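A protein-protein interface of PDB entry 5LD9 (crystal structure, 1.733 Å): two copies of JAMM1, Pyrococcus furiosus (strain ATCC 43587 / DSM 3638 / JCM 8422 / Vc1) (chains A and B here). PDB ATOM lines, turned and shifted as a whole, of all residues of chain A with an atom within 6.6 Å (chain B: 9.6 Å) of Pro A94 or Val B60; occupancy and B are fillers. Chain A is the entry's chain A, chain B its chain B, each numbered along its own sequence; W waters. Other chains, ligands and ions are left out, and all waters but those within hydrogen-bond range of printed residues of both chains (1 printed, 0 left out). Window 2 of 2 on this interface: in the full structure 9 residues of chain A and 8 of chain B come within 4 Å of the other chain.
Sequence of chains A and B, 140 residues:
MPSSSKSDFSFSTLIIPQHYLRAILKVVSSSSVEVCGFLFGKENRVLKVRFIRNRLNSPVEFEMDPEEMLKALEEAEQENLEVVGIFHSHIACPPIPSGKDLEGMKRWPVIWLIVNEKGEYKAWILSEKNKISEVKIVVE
The backbone carbonyl oxygen (O) of Cys A93 sits at hydrogen-bond distance from the side-chain amide nitrogen (ND2) of Asn A116, at 3.1 Å. The side-chain hydroxyl (OG) of Ser B58 lies within hydrogen-bond range of the backbone NH (N) of Val B60 (3.0 Å). ND1 of His A90 sits at hydrogen-bond distance from O of Pro A94, 2.9 Å away.
SG of Cys A93 is disulfide-bonded to SG of Cys B93. The backbone carbonyl oxygen (O) of Pro A97 is in hydrogen-bond range of the backbone NH (N) of Gly B99 (3.0 Å).
Hydrophobic or aromatic side chains of chain A that line the printed part of chain B: Pro A94. Hydrophobic or aromatic side chains of chain B that line the printed part of chain A: Val B60. Along chain B the printed residues that touch a printed residue of chain A span positions 60 to 99. Among the printed residues, 5 pairs touch across the chains. Among the printed residues, no Asp or Glu carboxylate lies within 4 Å of a Lys or Arg side-chain nitrogen of the other chain.
Ala A92 touches Cys B93, but with the chains exchanged Cys A93 does not touch Ala B92 (5.3 Å). Cys A93 touches its own counterpart, Cys B93. Pro A94 touches Cys B93, but with the chains exchanged Cys A93 does not touch Pro B94 (4.4 Å).
Of the printed residues of chain B, Pro A94 touches Val B60 (3.8 Å) and Cys B93 (3.8 Å). Ser B31 touches none of the printed residues of chain A. Of chain A, only Pro A94 (3.8 Å) comes within 4 Å of Val B60. Phe B62 touches none of the printed residues of chain A. Printed residues of chain A within 4 Å of Cys B93: Ala A92 (3.9 Å), Cys A93 (2.0 Å) and Pro A94 (3.8 Å). Of the printed residues of chain A, Gly B99 touches Pro A97. The nearest printed residue of chain B that does not touch Pro A94 is Ile B91 (5.9 Å). The nearest residue of chain A that does not touch Val B60 is Ile A96 (4.1 Å). The nearest printed residue of chain A that does not touch Gly B99 is Ile A96 (6.3 Å).
Ala A92 touches Cys B93 (O to SG, 3.9 Å). CG of Pro A94 touches CG1 of Val B60, 3.8 Å away. CD of Pro A94 touches SG of Cys B93 (3.8 Å).
Water W1 lies within hydrogen-bond range of the backbone carbonyl oxygen (O) of Pro A97 (2.6 Å), the backbone NH (N) of Lys B100 (3.0 Å) and the backbone NH (N) of Gly B99 (3.3 Å).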
ATOM      1  N   HIS A  90       8.845  17.153  -4.675  1.00  0.00           N
ATOM      2  CA  HIS A  90       9.312  16.678  -3.385  1.00  0.00           C
ATOM      3  C   HIS A  90      10.301  15.549  -3.614  1.00  0.00           C
ATOM      4  O   HIS A  90      10.226  14.840  -4.617  1.00  0.00           O
ATOM      5  CB  HIS A  90       8.161  16.160  -2.529  1.00  0.00           C
ATOM      6  CG  HIS A  90       7.198  17.227  -2.124  1.00  0.00           C
ATOM      7  ND1 HIS A  90       5.941  16.943  -1.636  1.00  0.00           N
ATOM      8  CD2 HIS A  90       7.306  18.575  -2.143  1.00  0.00           C
ATOM      9  CE1 HIS A  90       5.315  18.078  -1.375  1.00  0.00           C
ATOM     10  NE2 HIS A  90       6.127  19.081  -1.663  1.00  0.00           N
ATOM     11  N   ILE A  91      11.232  15.389  -2.682  1.00  0.00           N
ATOM     12  CA  ILE A  91      12.203  14.302  -2.739  1.00  0.00           C
ATOM     13  C   ILE A  91      11.885  13.341  -1.600  1.00  0.00           C
ATOM     14  O   ILE A  91      11.940  13.717  -0.423  1.00  0.00           O
ATOM     15  CB  ILE A  91      13.650  14.815  -2.658  1.00  0.00           C
ATOM     16  CG1 ILE A  91      13.922  15.783  -3.820  1.00  0.00           C
ATOM     17  CG2 ILE A  91      14.615  13.660  -2.743  1.00  0.00           C
ATOM     18  CD1 ILE A  91      15.311  16.408  -3.813  1.00  0.00           C
ATOM     19  N   ALA A  92      11.523  12.111  -1.956  1.00  0.00           N
ATOM     20  CA  ALA A  92      11.295  11.039  -0.988  1.00  0.00           C
ATOM     21  C   ALA A  92      10.123  11.347  -0.056  1.00  0.00           C
ATOM     22  O   ALA A  92      10.094  10.894   1.091  1.00  0.00           O
ATOM     23  CB  ALA A  92      12.559  10.751  -0.175  1.00  0.00           C
ATOM     24  N   CYS A  93       9.162  12.123  -0.534  1.00  0.00           N
ATOM     25  CA  CYS A  93       7.906  12.304   0.172  1.00  0.00           C
ATOM     26  C   CYS A  93       6.780  12.364  -0.848  1.00  0.00           C
ATOM     27  O   CYS A  93       7.012  12.588  -2.044  1.00  0.00           O
ATOM     28  CB  CYS A  93       7.909  13.555   1.070  1.00  0.00           C
ATOM     29  SG  CYS A  93       8.818  13.322   2.667  1.00  0.00           S
ATOM     30  N   PRO A  94       5.551  12.096  -0.413  1.00  0.00           N
ATOM     31  CA  PRO A  94       4.421  12.051  -1.365  1.00  0.00           C
ATOM     32  C   PRO A  94       4.179  13.404  -2.012  1.00  0.00           C
ATOM     33  O   PRO A  94       4.514  14.453  -1.443  1.00  0.00           O
ATOM     34  CB  PRO A  94       3.228  11.637  -0.489  1.00  0.00           C
ATOM     35  CG  PRO A  94       3.836  10.988   0.701  1.00  0.00           C
ATOM     36  CD  PRO A  94       5.138  11.682   0.939  1.00  0.00           C
ATOM     37  N   PRO A  95       3.580  13.423  -3.205  1.00  0.00           N
ATOM     38  CA  PRO A  95       3.326  14.691  -3.908  1.00  0.00           C
ATOM     39  C   PRO A  95       2.067  15.387  -3.397  1.00  0.00           C
ATOM     40  O   PRO A  95       1.099  15.617  -4.136  1.00  0.00           O
ATOM     41  CB  PRO A  95       3.205  14.231  -5.369  1.00  0.00           C
ATOM     42  CG  PRO A  95       2.617  12.867  -5.278  1.00  0.00           C
ATOM     43  CD  PRO A  95       3.167  12.252  -4.002  1.00  0.00           C
ATOM     44  N   ILE A  96       2.085  15.727  -2.108  1.00  0.00           N
ATOM     45  CA  ILE A  96       0.936  16.277  -1.391  1.00  0.00           C
ATOM     46  C   ILE A  96       1.373  17.603  -0.773  1.00  0.00           C
ATOM     47  O   ILE A  96       2.516  17.714  -0.321  1.00  0.00           O
ATOM     48  CB  ILE A  96       0.433  15.279  -0.332  1.00  0.00           C
ATOM     49  CG1 ILE A  96       0.081  13.940  -1.007  1.00  0.00           C
ATOM     50  CG2 ILE A  96      -0.776  15.810   0.390  1.00  0.00           C
ATOM     51  CD1 ILE A  96      -0.238  12.811  -0.053  1.00  0.00           C
ATOM     52  N   PRO A  97       0.526  18.633  -0.724  1.00  0.00           N
ATOM     53  CA  PRO A  97       1.008  19.945  -0.269  1.00  0.00           C
ATOM     54  C   PRO A  97       1.548  19.919   1.158  1.00  0.00           C
ATOM     55  O   PRO A  97       0.904  19.414   2.080  1.00  0.00           O
ATOM     56  CB  PRO A  97      -0.239  20.834  -0.366  1.00  0.00           C
ATOM     57  CG  PRO A  97      -1.078  20.183  -1.403  1.00  0.00           C
ATOM     58  CD  PRO A  97      -0.869  18.702  -1.189  1.00  0.00           C
ATOM     59  N   ILE A 114       2.435  18.751  -8.195  1.00  0.00           N
ATOM     60  CA  ILE A 114       3.533  18.272  -7.369  1.00  0.00           C
ATOM     61  C   ILE A 114       3.947  16.902  -7.878  1.00  0.00           C
ATOM     62  O   ILE A 114       3.092  16.047  -8.140  1.00  0.00           O
ATOM     63  CB  ILE A 114       3.159  18.216  -5.881  1.00  0.00           C
ATOM     64  CG1 ILE A 114       2.496  19.536  -5.462  1.00  0.00           C
ATOM     65  CG2 ILE A 114       4.403  17.907  -5.065  1.00  0.00           C
ATOM     66  CD1 ILE A 114       2.135  19.599  -3.956  1.00  0.00           C
ATOM     67  N   VAL A 115       5.256  16.699  -8.007  1.00  0.00           N
ATOM     68  CA  VAL A 115       5.830  15.436  -8.452  1.00  0.00           C
ATOM     69  C   VAL A 115       6.928  15.037  -7.476  1.00  0.00           C
ATOM     70  O   VAL A 115       7.371  15.835  -6.653  1.00  0.00           O
ATOM     71  CB  VAL A 115       6.388  15.518  -9.890  1.00  0.00           C
ATOM     72  CG1 VAL A 115       5.355  16.124 -10.833  1.00  0.00           C
ATOM     73  CG2 VAL A 115       7.688  16.316  -9.955  1.00  0.00           C
ATOM     74  N   ASN A 116       7.397  13.786  -7.591  1.00  0.00           N
ATOM     75  CA  ASN A 116       8.563  13.369  -6.826  1.00  0.00           C
ATOM     76  C   ASN A 116       9.452  12.485  -7.685  1.00  0.00           C
ATOM     77  O   ASN A 116       9.177  12.236  -8.869  1.00  0.00           O
ATOM     78  CB  ASN A 116       8.169  12.682  -5.506  1.00  0.00           C
ATOM     79  CG  ASN A 116       7.430  11.375  -5.698  1.00  0.00           C
ATOM     80  OD1 ASN A 116       7.492  10.742  -6.757  1.00  0.00           O
ATOM     81  ND2 ASN A 116       6.747  10.940  -4.644  1.00  0.00           N
ATOM     82  N   LYS A 118      10.037   9.409  -7.476  1.00  0.00           N
ATOM     83  CA  LYS A 118       9.478   8.097  -7.756  1.00  0.00           C
ATOM     84  C   LYS A 118       8.544   8.115  -8.956  1.00  0.00           C
ATOM     85  O   LYS A 118       7.885   7.110  -9.226  1.00  0.00           O
ATOM     86  CB  LYS A 118       8.728   7.575  -6.530  1.00  0.00           C
ATOM     87  CG  LYS A 118       9.601   7.472  -5.290  1.00  0.00           C
ATOM     88  CD  LYS A 118       8.785   7.170  -4.049  1.00  0.00           C
ATOM     89  CE  LYS A 118       9.601   7.411  -2.791  1.00  0.00           C
ATOM     90  NZ  LYS A 118       8.755   7.416  -1.567  1.00  0.00           N
ATOM     91  N   GLU A 120       5.826   9.883  -9.245  1.00  0.00           N
ATOM     92  CA  GLU A 120       4.459  10.156  -8.840  1.00  0.00           C
ATOM     93  C   GLU A 120       4.115  11.614  -9.106  1.00  0.00           C
ATOM     94  O   GLU A 120       4.976  12.498  -9.055  1.00  0.00           O
ATOM     95  CB  GLU A 120       4.280   9.816  -7.361  1.00  0.00           C
ATOM     96  CG  GLU A 120       4.464   8.325  -7.095  1.00  0.00           C
ATOM     97  CD  GLU A 120       4.704   7.986  -5.634  1.00  0.00           C
ATOM     98  OE1 GLU A 120       4.913   6.788  -5.340  1.00  0.00           O
ATOM     99  OE2 GLU A 120       4.694   8.900  -4.783  1.00  0.00           O
ATOM    100  N   SER B  31       3.273   0.487  12.939  1.00  0.00           N
ATOM    101  CA  SER B  31       2.065   0.789  12.187  1.00  0.00           C
ATOM    102  C   SER B  31       2.410   1.116  10.740  1.00  0.00           C
ATOM    103  O   SER B  31       3.352   1.866  10.468  1.00  0.00           O
ATOM    104  CB  SER B  31       1.311   1.958  12.830  1.00  0.00           C
ATOM    105  OG  SER B  31       0.165   2.296  12.071  1.00  0.00           O
ATOM    106  N   SER B  32       1.643   0.546   9.816  1.00  0.00           N
ATOM    107  CA  SER B  32       1.789   0.845   8.399  1.00  0.00           C
ATOM    108  C   SER B  32       0.914   2.009   7.954  1.00  0.00           C
ATOM    109  O   SER B  32       0.985   2.407   6.787  1.00  0.00           O
ATOM    110  CB  SER B  32       1.460  -0.396   7.560  1.00  0.00           C
ATOM    111  OG  SER B  32       0.102  -0.769   7.717  1.00  0.00           O
ATOM    112  N   VAL B  33       0.096   2.559   8.851  1.00  0.00           N
ATOM    113  CA  VAL B  33      -0.751   3.707   8.556  1.00  0.00           C
ATOM    114  C   VAL B  33      -0.504   4.780   9.613  1.00  0.00           C
ATOM    115  O   VAL B  33       0.081   4.529  10.668  1.00  0.00           O
ATOM    116  CB  VAL B  33      -2.248   3.335   8.510  1.00  0.00           C
ATOM    117  CG1 VAL B  33      -2.521   2.326   7.402  1.00  0.00           C
ATOM    118  CG2 VAL B  33      -2.707   2.800   9.861  1.00  0.00           C
ATOM    119  N   GLU B  34      -0.967   5.993   9.316  1.00  0.00           N
ATOM    120  CA  GLU B  34      -0.855   7.069  10.287  1.00  0.00           C
ATOM    121  C   GLU B  34      -1.657   6.715  11.532  1.00  0.00           C
ATOM    122  O   GLU B  34      -2.771   6.187  11.449  1.00  0.00           O
ATOM    123  CB  GLU B  34      -1.335   8.395   9.686  1.00  0.00           C
ATOM    124  CG  GLU B  34      -0.440   8.918   8.563  1.00  0.00           C
ATOM    125  CD  GLU B  34      -0.548  10.420   8.351  1.00  0.00           C
ATOM    126  OE1 GLU B  34      -1.479  11.047   8.900  1.00  0.00           O
ATOM    127  OE2 GLU B  34       0.308  10.981   7.632  1.00  0.00           O
ATOM    128  N   VAL B  35      -1.066   6.975  12.692  1.00  0.00           N
ATOM    129  CA  VAL B  35      -1.716   6.774  13.973  1.00  0.00           C
ATOM    130  C   VAL B  35      -2.186   8.136  14.470  1.00  0.00           C
ATOM    131  O   VAL B  35      -1.669   9.175  14.067  1.00  0.00           O
ATOM    132  CB  VAL B  35      -0.751   6.099  14.980  1.00  0.00           C
ATOM    133  CG1 VAL B  35      -1.380   5.963  16.359  1.00  0.00           C
ATOM    134  CG2 VAL B  35      -0.316   4.732  14.457  1.00  0.00           C
ATOM    135  N   ASN B  54      -7.769   5.457  13.090  1.00  0.00           N
ATOM    136  CA  ASN B  54      -7.670   6.259  11.870  1.00  0.00           C
ATOM    137  C   ASN B  54      -8.619   5.659  10.850  1.00  0.00           C
ATOM    138  O   ASN B  54      -8.318   4.633  10.238  1.00  0.00           O
ATOM    139  CB  ASN B  54      -6.235   6.264  11.353  1.00  0.00           C
ATOM    140  CG  ASN B  54      -6.076   7.011  10.046  1.00  0.00           C
ATOM    141  OD1 ASN B  54      -7.015   7.621   9.530  1.00  0.00           O
ATOM    142  ND2 ASN B  54      -4.864   6.992   9.511  1.00  0.00           N
ATOM    143  N   LEU B  56      -9.305   6.481   7.978  1.00  0.00           N
ATOM    144  CA  LEU B  56      -8.844   6.500   6.595  1.00  0.00           C
ATOM    145  C   LEU B  56      -7.893   5.354   6.276  1.00  0.00           C
ATOM    146  O   LEU B  56      -7.597   5.132   5.096  1.00  0.00           O
ATOM    147  CB  LEU B  56      -8.164   7.839   6.267  1.00  0.00           C
ATOM    148  CG  LEU B  56      -9.027   9.097   6.454  1.00  0.00           C
ATOM    149  CD1 LEU B  56      -8.309  10.335   5.930  1.00  0.00           C
ATOM    150  CD2 LEU B  56     -10.376   8.954   5.760  1.00  0.00           C
ATOM    151  N   ASN B  57      -7.424   4.621   7.285  1.00  0.00           N
ATOM    152  CA  ASN B  57      -6.551   3.469   7.081  1.00  0.00           C
ATOM    153  C   ASN B  57      -5.447   3.784   6.077  1.00  0.00           C
ATOM    154  O   ASN B  57      -5.190   3.021   5.145  1.00  0.00           O
ATOM    155  CB  ASN B  57      -7.359   2.255   6.615  1.00  0.00           C
ATOM    156  CG  ASN B  57      -8.304   1.753   7.664  1.00  0.00           C
ATOM    157  OD1 ASN B  57      -7.877   1.234   8.696  1.00  0.00           O
ATOM    158  ND2 ASN B  57      -9.598   1.901   7.418  1.00  0.00           N
ATOM    159  N   SER B  58      -4.786   4.926   6.268  1.00  0.00           N
ATOM    160  CA  SER B  58      -3.920   5.453   5.221  1.00  0.00           C
ATOM    161  C   SER B  58      -2.533   5.786   5.750  1.00  0.00           C
ATOM    162  O   SER B  58      -2.404   6.299   6.867  1.00  0.00           O
ATOM    163  CB  SER B  58      -4.518   6.721   4.603  1.00  0.00           C
ATOM    164  OG  SER B  58      -3.527   7.420   3.864  1.00  0.00           O
ATOM    165  N   PRO B  59      -1.483   5.549   4.959  1.00  0.00           N
ATOM    166  CA  PRO B  59      -0.133   5.943   5.368  1.00  0.00           C
ATOM    167  C   PRO B  59       0.223   7.393   5.081  1.00  0.00           C
ATOM    168  O   PRO B  59       1.371   7.777   5.329  1.00  0.00           O
ATOM    169  CB  PRO B  59       0.753   4.998   4.546  1.00  0.00           C
ATOM    170  CG  PRO B  59      -0.002   4.789   3.305  1.00  0.00           C
ATOM    171  CD  PRO B  59      -1.465   4.801   3.687  1.00  0.00           C
ATOM    172  N   VAL B  60      -0.705   8.212   4.577  1.00  0.00           N
ATOM    173  CA  VAL B  60      -0.413   9.605   4.251  1.00  0.00           C
ATOM    174  C   VAL B  60      -1.454  10.579   4.783  1.00  0.00           C
ATOM    175  O   VAL B  60      -1.327  11.784   4.552  1.00  0.00           O
ATOM    176  CB  VAL B  60      -0.235   9.808   2.730  1.00  0.00           C
ATOM    177  CG1 VAL B  60       0.985   9.053   2.233  1.00  0.00           C
ATOM    178  CG2 VAL B  60      -1.482   9.379   1.964  1.00  0.00           C
ATOM    179  N   GLU B  61      -2.472  10.115   5.503  1.00  0.00           N
ATOM    180  CA  GLU B  61      -3.413  11.035   6.134  1.00  0.00           C
ATOM    181  C   GLU B  61      -4.157  10.304   7.243  1.00  0.00           C
ATOM    182  O   GLU B  61      -4.100   9.080   7.352  1.00  0.00           O
ATOM    183  CB  GLU B  61      -4.390  11.619   5.111  1.00  0.00           C
ATOM    184  CG  GLU B  61      -5.180  10.575   4.357  1.00  0.00           C
ATOM    185  CD  GLU B  61      -6.179  11.189   3.387  1.00  0.00           C
ATOM    186  OE1 GLU B  61      -6.577  12.363   3.591  1.00  0.00           O
ATOM    187  OE2 GLU B  61      -6.563  10.493   2.425  1.00  0.00           O
ATOM    188  N   PHE B  62      -4.854  11.076   8.073  1.00  0.00           N
ATOM    189  CA  PHE B  62      -5.655  10.499   9.142  1.00  0.00           C
ATOM    190  C   PHE B  62      -6.928  11.310   9.335  1.00  0.00           C
ATOM    191  O   PHE B  62      -7.000  12.494   8.995  1.00  0.00           O
ATOM    192  CB  PHE B  62      -4.895  10.418  10.477  1.00  0.00           C
ATOM    193  CG  PHE B  62      -4.835  11.726  11.228  1.00  0.00           C
ATOM    194  CD1 PHE B  62      -3.878  12.679  10.917  1.00  0.00           C
ATOM    195  CD2 PHE B  62      -5.745  12.009  12.230  1.00  0.00           C
ATOM    196  CE1 PHE B  62      -3.833  13.880  11.590  1.00  0.00           C
ATOM    197  CE2 PHE B  62      -5.703  13.216  12.902  1.00  0.00           C
ATOM    198  CZ  PHE B  62      -4.743  14.144  12.589  1.00  0.00           C
ATOM    199  N   GLU B  63      -7.933  10.625   9.870  1.00  0.00           N
ATOM    200  CA  GLU B  63      -9.201  11.186  10.299  1.00  0.00           C
ATOM    201  C   GLU B  63      -9.687  10.301  11.440  1.00  0.00           C
ATOM    202  O   GLU B  63      -9.726   9.080  11.292  1.00  0.00           O
ATOM    203  CB  GLU B  63     -10.198  11.195   9.140  1.00  0.00           C
ATOM    204  CG  GLU B  63     -11.437  12.022   9.322  1.00  0.00           C
ATOM    205  CD  GLU B  63     -12.231  12.093   8.025  1.00  0.00           C
ATOM    206  OE1 GLU B  63     -13.234  11.365   7.905  1.00  0.00           O
ATOM    207  OE2 GLU B  63     -11.823  12.851   7.120  1.00  0.00           O
ATOM    208  N   HIS B  88      -0.490  12.670  16.158  1.00  0.00           N
ATOM    209  CA  HIS B  88      -0.574  11.743  15.038  1.00  0.00           C
ATOM    210  C   HIS B  88       0.834  11.516  14.512  1.00  0.00           C
ATOM    211  O   HIS B  88       1.785  12.198  14.900  1.00  0.00           O
ATOM    212  CB  HIS B  88      -1.528  12.233  13.936  1.00  0.00           C
ATOM    213  CG  HIS B  88      -0.966  13.305  13.052  1.00  0.00           C
ATOM    214  ND1 HIS B  88      -0.897  14.630  13.431  1.00  0.00           N
ATOM    215  CD2 HIS B  88      -0.503  13.255  11.780  1.00  0.00           C
ATOM    216  CE1 HIS B  88      -0.389  15.343  12.438  1.00  0.00           C
ATOM    217  NE2 HIS B  88      -0.135  14.530  11.429  1.00  0.00           N
ATOM    218  N   SER B  89       0.958  10.523  13.647  1.00  0.00           N
ATOM    219  CA  SER B  89       2.237  10.152  13.081  1.00  0.00           C
ATOM    220  C   SER B  89       2.277  10.392  11.578  1.00  0.00           C
ATOM    221  O   SER B  89       1.253  10.399  10.888  1.00  0.00           O
ATOM    222  CB  SER B  89       2.555   8.679  13.362  1.00  0.00           C
ATOM    223  OG  SER B  89       1.612   7.817  12.744  1.00  0.00           O
ATOM    224  N   HIS B  90       3.498  10.589  11.096  1.00  0.00           N
ATOM    225  CA  HIS B  90       3.856  10.515   9.691  1.00  0.00           C
ATOM    226  C   HIS B  90       4.714   9.283   9.471  1.00  0.00           C
ATOM    227  O   HIS B  90       5.448   8.852  10.361  1.00  0.00           O
ATOM    228  CB  HIS B  90       4.638  11.751   9.253  1.00  0.00           C
ATOM    229  CG  HIS B  90       3.813  12.995   9.228  1.00  0.00           C
ATOM    230  ND1 HIS B  90       4.370  14.252   9.130  1.00  0.00           N
ATOM    231  CD2 HIS B  90       2.472  13.174   9.275  1.00  0.00           C
ATOM    232  CE1 HIS B  90       3.402  15.153   9.119  1.00  0.00           C
ATOM    233  NE2 HIS B  90       2.244  14.523   9.211  1.00  0.00           N
ATOM    234  N   ILE B  91       4.605   8.710   8.283  1.00  0.00           N
ATOM    235  CA  ILE B  91       5.471   7.615   7.875  1.00  0.00           C
ATOM    236  C   ILE B  91       6.563   8.209   7.001  1.00  0.00           C
ATOM    237  O   ILE B  91       6.281   8.772   5.937  1.00  0.00           O
ATOM    238  CB  ILE B  91       4.679   6.512   7.156  1.00  0.00           C
ATOM    239  CG1 ILE B  91       3.874   5.728   8.199  1.00  0.00           C
ATOM    240  CG2 ILE B  91       5.609   5.577   6.384  1.00  0.00           C
ATOM    241  CD1 ILE B  91       2.881   4.751   7.636  1.00  0.00           C
ATOM    242  N   ALA B  92       7.801   8.134   7.490  1.00  0.00           N
ATOM    243  CA  ALA B  92       8.997   8.557   6.768  1.00  0.00           C
ATOM    244  C   ALA B  92       9.234  10.065   6.828  1.00  0.00           C
ATOM    245  O   ALA B  92      10.354  10.502   7.111  1.00  0.00           O
ATOM    246  CB  ALA B  92       8.942   8.098   5.307  1.00  0.00           C
ATOM    247  N   CYS B  93       8.210  10.874   6.584  1.00  0.00           N
ATOM    248  CA  CYS B  93       8.496  12.288   6.433  1.00  0.00           C
ATOM    249  C   CYS B  93       8.607  12.961   7.806  1.00  0.00           C
ATOM    250  O   CYS B  93       8.290  12.377   8.844  1.00  0.00           O
ATOM    251  CB  CYS B  93       7.463  12.904   5.490  1.00  0.00           C
ATOM    252  SG  CYS B  93       7.626  12.124   3.813  1.00  0.00           S
ATOM    253  N   PRO B  94       9.142  14.182   7.838  1.00  0.00           N
ATOM    254  CA  PRO B  94       9.448  14.833   9.128  1.00  0.00           C
ATOM    255  C   PRO B  94       8.186  15.165   9.903  1.00  0.00           C
ATOM    256  O   PRO B  94       7.096  15.286   9.323  1.00  0.00           O
ATOM    257  CB  PRO B  94      10.195  16.111   8.717  1.00  0.00           C
ATOM    258  CG  PRO B  94      10.642  15.884   7.325  1.00  0.00           C
ATOM    259  CD  PRO B  94       9.620  14.988   6.702  1.00  0.00           C
ATOM    260  N   SER B  98       1.616  19.006   7.612  1.00  0.00           N
ATOM    261  CA  SER B  98       1.258  19.092   6.206  1.00  0.00           C
ATOM    262  C   SER B  98       0.265  20.230   5.991  1.00  0.00           C
ATOM    263  O   SER B  98      -0.227  20.845   6.936  1.00  0.00           O
ATOM    264  CB  SER B  98       0.628  17.783   5.738  1.00  0.00           C
ATOM    265  OG  SER B  98      -0.610  17.573   6.405  1.00  0.00           O
ATOM    266  N   GLY B  99      -0.057  20.500   4.727  1.00  0.00           N
ATOM    267  CA  GLY B  99      -1.111  21.467   4.466  1.00  0.00           C
ATOM    268  C   GLY B  99      -2.437  21.047   5.078  1.00  0.00           C
ATOM    269  O   GLY B  99      -3.135  21.860   5.691  1.00  0.00           O
ATOM    270  N   LYS B 100      -2.804  19.774   4.918  1.00  0.00           N
ATOM    271  CA  LYS B 100      -4.036  19.276   5.527  1.00  0.00           C
ATOM    272  C   LYS B 100      -3.960  19.311   7.050  1.00  0.00           C
ATOM    273  O   LYS B 100      -4.974  19.566   7.715  1.00  0.00           O
ATOM    274  CB  LYS B 100      -4.334  17.857   5.027  1.00  0.00           C
ATOM    275  CG  LYS B 100      -4.584  17.752   3.512  1.00  0.00           C
ATOM    276  CD  LYS B 100      -5.956  17.162   3.193  1.00  0.00           C
ATOM    277  CE  LYS B 100      -6.166  16.951   1.695  1.00  0.00           C
ATOM    278  NZ  LYS B 100      -5.313  15.859   1.135  1.00  0.00           N
ATOM    279  N   ASP B 101      -2.769  19.103   7.620  1.00  0.00           N
ATOM    280  CA  ASP B 101      -2.605  19.245   9.065  1.00  0.00           C
ATOM    281  C   ASP B 101      -2.913  20.669   9.522  1.00  0.00           C
ATOM    282  O   ASP B 101      -3.573  20.867  10.550  1.00  0.00           O
ATOM    283  CB  ASP B 101      -1.185  18.861   9.487  1.00  0.00           C
ATOM    284  CG  ASP B 101      -0.923  17.350   9.443  1.00  0.00           C
ATOM    285  OD1 ASP B 101      -1.882  16.547   9.406  1.00  0.00           O
ATOM    286  OD2 ASP B 101       0.265  16.963   9.453  1.00  0.00           O
HETATM  287  O   HOH W   1      -1.421  18.338   2.663  1.00  0.00           O
